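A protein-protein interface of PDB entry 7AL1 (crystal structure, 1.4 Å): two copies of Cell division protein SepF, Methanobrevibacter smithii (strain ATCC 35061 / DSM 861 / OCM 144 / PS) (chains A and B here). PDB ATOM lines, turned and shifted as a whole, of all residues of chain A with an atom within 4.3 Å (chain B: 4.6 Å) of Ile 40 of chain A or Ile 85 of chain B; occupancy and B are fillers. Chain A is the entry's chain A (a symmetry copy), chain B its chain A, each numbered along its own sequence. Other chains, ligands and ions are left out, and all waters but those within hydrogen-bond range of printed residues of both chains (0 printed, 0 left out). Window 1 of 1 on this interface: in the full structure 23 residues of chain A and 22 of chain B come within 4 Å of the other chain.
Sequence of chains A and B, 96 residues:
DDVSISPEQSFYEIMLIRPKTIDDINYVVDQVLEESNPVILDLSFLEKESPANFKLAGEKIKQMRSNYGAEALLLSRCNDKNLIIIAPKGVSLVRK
The backbone NH (N) of Leu 93 of chain B is in hydrogen-bond range of the side-chain carboxylate (OE1) of Glu 71 of chain B (3.0 Å). The backbone NH (N) of Leu 73 of chain B sits at hydrogen-bond distance from the backbone carbonyl oxygen (O) of Ile 85 of chain B (2.9 Å). N of Leu 75 of chain B lies within hydrogen-bond range of O of Leu 83 of chain B (2.8 Å). The backbone NH (N) of Ile 40 of chain A sits at hydrogen-bond distance from the backbone carbonyl oxygen (O) of Met 15 of chain A, 2.7 Å away. The backbone carbonyl oxygen (O) of Ile 40 of chain A is in hydrogen-bond range of the backbone NH (N) of Ile 17 of chain A.
Ile 14 of chain A touches Ile 85 of chain B (CD1 to CD1, 3.98 Å). O of Ile 14 of chain A touches CA of Leu 93 of chain B (3.4 Å). Leu 16 of chain A touches Leu 73 of chain B (CD2 to CD2, 3.8 Å). Leu 75 of chain B touches Leu 16 of chain A. Ile 40 of chain A touches Ile 85 of chain B (CD1 to CD1, 3.8 Å). CD1 of Ile 85 of chain A touches CD1 of Ile 40 of chain B, 3.8 Å away.
Hydrophobic or aromatic side chains of chain A that line the printed part of chain B: Ile 14, Leu 16, Ile 40 and Ile 85. Among the printed residues, no Asp or Glu carboxylate lies within 4 Å of a Lys or Arg side-chain nitrogen of the other chain.
Of the printed residues of chain B, Ile 14 of chain A touches Ile 85 and Leu 93. Printed residues of chain B within 4 Å of Ile 40 of chain A: Ile 85. Printed residues of chain A within 4 Å of Ile 40 of chain B: Ile 85 (3.8 Å). Printed residues of chain A within 4 Å of Leu 75 of chain B: Leu 16. Ile 86 of chain B touches none of the printed residues of chain A. The nearest residue of chain B that does not touch Ile 40 of chain A is Leu 75 of chain B (4.2 Å). The nearest printed residue of chain B that does not touch Ile 14 of chain A is Ala 87 of chain B (5.4 Å).
Ile 40 of chain A touches Ile 85 of chain B, and with the chains exchanged Ile 85 of chain A touches Ile 40 of chain B. 4 positions are printed for both chains.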
ATOM      1  N   ILE A  14       2.926 -16.388  15.811  1.00  0.00           N
ATOM      2  CA  ILE A  14       3.053 -15.578  14.620  1.00  0.00           C
ATOM      3  C   ILE A  14       2.539 -16.405  13.459  1.00  0.00           C
ATOM      4  O   ILE A  14       3.058 -17.493  13.181  1.00  0.00           O
ATOM      5  CB  ILE A  14       4.493 -15.139  14.360  1.00  0.00           C
ATOM      6  CG1 ILE A  14       4.966 -14.241  15.504  1.00  0.00           C
ATOM      7  CG2 ILE A  14       4.548 -14.431  13.028  1.00  0.00           C
ATOM      8  CD1 ILE A  14       6.447 -13.931  15.448  1.00  0.00           C
ATOM      9  N   MET A  15       1.548 -15.891  12.747  1.00  0.00           N
ATOM     10  CA  MET A  15       0.893 -16.646  11.699  1.00  0.00           C
ATOM     11  C   MET A  15       1.487 -16.287  10.358  1.00  0.00           C
ATOM     12  O   MET A  15       1.797 -15.122  10.094  1.00  0.00           O
ATOM     13  CB  MET A  15      -0.604 -16.338  11.641  1.00  0.00           C
ATOM     14  CG  MET A  15      -1.266 -16.170  12.977  1.00  0.00           C
ATOM     15  SD  MET A  15      -1.235 -17.714  13.905  1.00  0.00           S
ATOM     16  CE  MET A  15      -2.218 -18.726  12.811  1.00  0.00           C
ATOM     17  N   LEU A  16       1.639 -17.272   9.497  1.00  0.00           N
ATOM     18  CA  LEU A  16       2.106 -17.068   8.134  1.00  0.00           C
ATOM     19  C   LEU A  16       0.996 -17.517   7.208  1.00  0.00           C
ATOM     20  O   LEU A  16       0.534 -18.658   7.289  1.00  0.00           O
ATOM     21  CB  LEU A  16       3.384 -17.864   7.866  1.00  0.00           C
ATOM     22  CG  LEU A  16       4.539 -17.386   8.774  1.00  0.00           C
ATOM     23  CD1 LEU A  16       4.797 -18.451   9.822  1.00  0.00           C
ATOM     24  CD2 LEU A  16       5.811 -17.108   8.021  1.00  0.00           C
ATOM     25  N   ILE A  17       0.553 -16.623   6.333  1.00  0.00           N
ATOM     26  CA  ILE A  17      -0.645 -16.843   5.517  1.00  0.00           C
ATOM     27  C   ILE A  17      -0.418 -16.236   4.133  1.00  0.00           C
ATOM     28  O   ILE A  17       0.018 -15.079   4.058  1.00  0.00           O
ATOM     29  CB  ILE A  17      -1.853 -16.169   6.212  1.00  0.00           C
ATOM     30  CG1 ILE A  17      -2.033 -16.621   7.681  1.00  0.00           C
ATOM     31  CG2 ILE A  17      -3.148 -16.456   5.475  1.00  0.00           C
ATOM     32  CD1 ILE A  17      -3.092 -15.846   8.548  1.00  0.00           C
ATOM     33  N   PRO A  38       0.536 -11.476  15.488  1.00  0.00           N
ATOM     34  CA  PRO A  38       1.131 -10.937  14.267  1.00  0.00           C
ATOM     35  C   PRO A  38       0.922 -11.893  13.108  1.00  0.00           C
ATOM     36  O   PRO A  38       0.848 -13.118  13.283  1.00  0.00           O
ATOM     37  CB  PRO A  38       2.619 -10.831  14.624  1.00  0.00           C
ATOM     38  CG  PRO A  38       2.669 -10.848  16.117  1.00  0.00           C
ATOM     39  CD  PRO A  38       1.528 -11.720  16.551  1.00  0.00           C
ATOM     40  N   VAL A  39       0.845 -11.332  11.909  1.00  0.00           N
ATOM     41  CA  VAL A  39       0.683 -12.116  10.692  1.00  0.00           C
ATOM     42  C   VAL A  39       1.739 -11.684   9.697  1.00  0.00           C
ATOM     43  O   VAL A  39       1.879 -10.489   9.400  1.00  0.00           O
ATOM     44  CB  VAL A  39      -0.728 -11.965  10.083  1.00  0.00           C
ATOM     45  CG1 VAL A  39      -0.828 -12.740   8.763  1.00  0.00           C
ATOM     46  CG2 VAL A  39      -1.785 -12.429  11.064  1.00  0.00           C
ATOM     47  N   ILE A  40       2.509 -12.633   9.206  1.00  0.00           N
ATOM     48  CA  ILE A  40       3.369 -12.410   8.041  1.00  0.00           C
ATOM     49  C   ILE A  40       2.547 -12.815   6.826  1.00  0.00           C
ATOM     50  O   ILE A  40       2.252 -13.998   6.628  1.00  0.00           O
ATOM     51  CB  ILE A  40       4.701 -13.161   8.130  1.00  0.00           C
ATOM     52  CG1 ILE A  40       5.506 -12.648   9.341  1.00  0.00           C
ATOM     53  CG2 ILE A  40       5.458 -12.965   6.833  1.00  0.00           C
ATOM     54  CD1 ILE A  40       6.730 -13.485   9.688  1.00  0.00           C
ATOM     55  N   LEU A  41       2.102 -11.821   6.069  1.00  0.00           N
ATOM     56  CA  LEU A  41       1.113 -11.959   5.024  1.00  0.00           C
ATOM     57  C   LEU A  41       1.836 -11.937   3.685  1.00  0.00           C
ATOM     58  O   LEU A  41       2.621 -11.018   3.424  1.00  0.00           O
ATOM     59  CB  LEU A  41       0.210 -10.710   5.131  1.00  0.00           C
ATOM     60  CG  LEU A  41      -1.001 -10.589   4.245  1.00  0.00           C
ATOM     61  CD1 LEU A  41      -1.920 -11.721   4.482  1.00  0.00           C
ATOM     62  CD2 LEU A  41      -1.710  -9.286   4.557  1.00  0.00           C
ATOM     63  N   ASP A  42       1.552 -12.912   2.816  1.00  0.00           N
ATOM     64  CA  ASP A  42       2.087 -12.943   1.459  1.00  0.00           C
ATOM     65  C   ASP A  42       0.928 -12.641   0.504  1.00  0.00           C
ATOM     66  O   ASP A  42       0.046 -13.480   0.321  1.00  0.00           O
ATOM     67  CB  ASP A  42       2.717 -14.295   1.118  1.00  0.00           C
ATOM     68  CG  ASP A  42       3.248 -14.351  -0.279  1.00  0.00           C
ATOM     69  OD1 ASP A  42       3.192 -13.358  -1.012  1.00  0.00           O
ATOM     70  OD2 ASP A  42       3.743 -15.453  -0.686  1.00  0.00           O
ATOM     71  N   ILE A  84       4.345  -8.760   3.884  1.00  0.00           N
ATOM     72  CA  ILE A  84       4.074  -7.681   4.837  1.00  0.00           C
ATOM     73  C   ILE A  84       3.899  -8.291   6.216  1.00  0.00           C
ATOM     74  O   ILE A  84       3.319  -9.372   6.340  1.00  0.00           O
ATOM     75  CB  ILE A  84       2.783  -6.941   4.442  1.00  0.00           C
ATOM     76  CG1 ILE A  84       2.891  -6.403   3.022  1.00  0.00           C
ATOM     77  CG2 ILE A  84       2.395  -5.810   5.397  1.00  0.00           C
ATOM     78  CD1 ILE A  84       1.544  -6.246   2.335  1.00  0.00           C
ATOM     79  N   ILE A  85       4.440  -7.668   7.252  1.00  0.00           N
ATOM     80  CA  ILE A  85       4.109  -8.067   8.609  1.00  0.00           C
ATOM     81  C   ILE A  85       3.092  -7.120   9.207  1.00  0.00           C
ATOM     82  O   ILE A  85       3.276  -5.896   9.173  1.00  0.00           O
ATOM     83  CB  ILE A  85       5.335  -8.220   9.529  1.00  0.00           C
ATOM     84  CG1 ILE A  85       4.856  -8.779  10.886  1.00  0.00           C
ATOM     85  CG2 ILE A  85       6.111  -6.948   9.662  1.00  0.00           C
ATOM     86  CD1 ILE A  85       5.924  -9.398  11.724  1.00  0.00           C
ATOM     87  N   VAL B  39      13.118 -12.220  15.796  1.00  0.00           N
ATOM     88  CA  VAL B  39      13.932 -11.333  14.979  1.00  0.00           C
ATOM     89  C   VAL B  39      13.662 -11.640  13.521  1.00  0.00           C
ATOM     90  O   VAL B  39      13.756 -12.797  13.089  1.00  0.00           O
ATOM     91  CB  VAL B  39      15.439 -11.469  15.290  1.00  0.00           C
ATOM     92  CG1 VAL B  39      16.262 -10.578  14.350  1.00  0.00           C
ATOM     93  CG2 VAL B  39      15.716 -11.129  16.740  1.00  0.00           C
ATOM     94  N   ILE B  40      13.292 -10.627  12.764  1.00  0.00           N
ATOM     95  CA  ILE B  40      13.274 -10.715  11.301  1.00  0.00           C
ATOM     96  C   ILE B  40      14.636 -10.224  10.833  1.00  0.00           C
ATOM     97  O   ILE B  40      14.956  -9.038  10.954  1.00  0.00           O
ATOM     98  CB  ILE B  40      12.115  -9.937  10.672  1.00  0.00           C
ATOM     99  CG1 ILE B  40      10.774 -10.536  11.138  1.00  0.00           C
ATOM    100  CG2 ILE B  40      12.256  -9.990   9.165  1.00  0.00           C
ATOM    101  CD1 ILE B  40       9.551  -9.698  10.785  1.00  0.00           C
ATOM    102  N   GLU B  71      13.153 -21.493  16.463  1.00  0.00           N
ATOM    103  CA  GLU B  71      12.816 -21.805  15.081  1.00  0.00           C
ATOM    104  C   GLU B  71      13.454 -20.770  14.163  1.00  0.00           C
ATOM    105  O   GLU B  71      13.671 -19.636  14.565  1.00  0.00           O
ATOM    106  CB  GLU B  71      11.295 -21.716  14.867  1.00  0.00           C
ATOM    107  CG  GLU B  71      10.424 -22.710  15.633  1.00  0.00           C
ATOM    108  CD  GLU B  71       8.938 -22.582  15.259  1.00  0.00           C
ATOM    109  OE1 GLU B  71       8.232 -21.754  15.876  1.00  0.00           O
ATOM    110  OE2 GLU B  71       8.479 -23.301  14.342  1.00  0.00           O
ATOM    111  N   ALA B  72      13.793 -21.160  12.938  1.00  0.00           N
ATOM    112  CA  ALA B  72      14.337 -20.208  11.971  1.00  0.00           C
ATOM    113  C   ALA B  72      13.783 -20.579  10.616  1.00  0.00           C
ATOM    114  O   ALA B  72      14.102 -21.659  10.109  1.00  0.00           O
ATOM    115  CB  ALA B  72      15.863 -20.240  11.938  1.00  0.00           C
ATOM    116  N   LEU B  73      12.987 -19.699  10.029  1.00  0.00           N
ATOM    117  CA  LEU B  73      12.232 -19.974   8.816  1.00  0.00           C
ATOM    118  C   LEU B  73      12.589 -18.949   7.762  1.00  0.00           C
ATOM    119  O   LEU B  73      12.472 -17.736   8.000  1.00  0.00           O
ATOM    120  CB  LEU B  73      10.729 -19.930   9.117  1.00  0.00           C
ATOM    121  CG  LEU B  73       9.803 -20.291   7.966  1.00  0.00           C
ATOM    122  CD1 LEU B  73       9.902 -21.775   7.631  1.00  0.00           C
ATOM    123  CD2 LEU B  73       8.366 -19.925   8.305  1.00  0.00           C
ATOM    124  N   LEU B  75      12.037 -16.575   4.857  1.00  0.00           N
ATOM    125  CA  LEU B  75      10.884 -15.850   4.328  1.00  0.00           C
ATOM    126  C   LEU B  75      11.033 -15.512   2.851  1.00  0.00           C
ATOM    127  O   LEU B  75      10.128 -15.819   2.062  1.00  0.00           O
ATOM    128  CB  LEU B  75      10.658 -14.567   5.137  1.00  0.00           C
ATOM    129  CG  LEU B  75      10.334 -14.729   6.602  1.00  0.00           C
ATOM    130  CD1 LEU B  75      10.156 -13.396   7.295  1.00  0.00           C
ATOM    131  CD2 LEU B  75       9.091 -15.596   6.786  1.00  0.00           C
ATOM    132  N   LEU B  83      15.817 -12.655   3.923  1.00  0.00           N
ATOM    133  CA  LEU B  83      15.024 -12.454   5.135  1.00  0.00           C
ATOM    134  C   LEU B  83      14.666 -13.797   5.763  1.00  0.00           C
ATOM    135  O   LEU B  83      14.050 -14.653   5.126  1.00  0.00           O
ATOM    136  CB  LEU B  83      13.724 -11.695   4.815  1.00  0.00           C
ATOM    137  CG  LEU B  83      13.845 -10.287   4.282  1.00  0.00           C
ATOM    138  CD1 LEU B  83      12.420  -9.690   4.214  1.00  0.00           C
ATOM    139  CD2 LEU B  83      14.750  -9.434   5.115  1.00  0.00           C
ATOM    140  N   ILE B  84      14.999 -13.934   7.034  1.00  0.00           N
ATOM    141  CA  ILE B  84      14.698 -15.105   7.862  1.00  0.00           C
ATOM    142  C   ILE B  84      14.023 -14.631   9.136  1.00  0.00           C
ATOM    143  O   ILE B  84      14.391 -13.584   9.674  1.00  0.00           O
ATOM    144  CB  ILE B  84      16.000 -15.843   8.223  1.00  0.00           C
ATOM    145  CG1 ILE B  84      16.752 -16.244   6.961  1.00  0.00           C
ATOM    146  CG2 ILE B  84      15.796 -17.069   9.116  1.00  0.00           C
ATOM    147  CD1 ILE B  84      18.251 -16.377   7.171  1.00  0.00           C
ATOM    148  N   ILE B  85      13.001 -15.331   9.604  1.00  0.00           N
ATOM    149  CA  ILE B  85      12.470 -15.069  10.932  1.00  0.00           C
ATOM    150  C   ILE B  85      12.980 -16.097  11.917  1.00  0.00           C
ATOM    151  O   ILE B  85      12.886 -17.307  11.670  1.00  0.00           O
ATOM    152  CB  ILE B  85      10.935 -14.966  10.979  1.00  0.00           C
ATOM    153  CG1 ILE B  85      10.522 -14.549  12.407  1.00  0.00           C
ATOM    154  CG2 ILE B  85      10.263 -16.221  10.518  1.00  0.00           C
ATOM    155  CD1 ILE B  85       9.147 -13.978  12.523  1.00  0.00           C
ATOM    156  N   ILE B  86      13.557 -15.629  13.009  1.00  0.00           N
ATOM    157  CA  ILE B  86      13.979 -16.480  14.109  1.00  0.00           C
ATOM    158  C   ILE B  86      13.013 -16.262  15.261  1.00  0.00           C
ATOM    159  O   ILE B  86      12.903 -15.152  15.782  1.00  0.00           O
ATOM    160  CB  ILE B  86      15.416 -16.160  14.551  1.00  0.00           C
ATOM    161  CG1 ILE B  86      16.378 -16.329  13.383  1.00  0.00           C
ATOM    162  CG2 ILE B  86      15.810 -17.037  15.743  1.00  0.00           C
ATOM    163  CD1 ILE B  86      17.700 -15.685  13.634  1.00  0.00           C
ATOM    164  N   ALA B  87      12.347 -17.322  15.695  1.00  0.00           N
ATOM    165  CA  ALA B  87      11.373 -17.231  16.759  1.00  0.00           C
ATOM    166  C   ALA B  87      11.900 -17.948  17.983  1.00  0.00           C
ATOM    167  O   ALA B  87      12.317 -19.105  17.881  1.00  0.00           O
ATOM    168  CB  ALA B  87      10.060 -17.874  16.319  1.00  0.00           C
ATOM    169  N   LEU B  93       5.731 -20.235  15.344  1.00  0.00           N
ATOM    170  CA  LEU B  93       5.335 -19.932  13.977  1.00  0.00           C
ATOM    171  C   LEU B  93       4.262 -20.924  13.577  1.00  0.00           C
ATOM    172  O   LEU B  93       4.374 -22.118  13.845  1.00  0.00           O
ATOM    173  CB  LEU B  93       6.536 -20.079  13.053  1.00  0.00           C
ATOM    174  CG  LEU B  93       7.713 -19.200  13.422  1.00  0.00           C
ATOM    175  CD1 LEU B  93       8.839 -19.428  12.459  1.00  0.00           C
ATOM    176  CD2 LEU B  93       7.323 -17.732  13.418  1.00  0.00           C
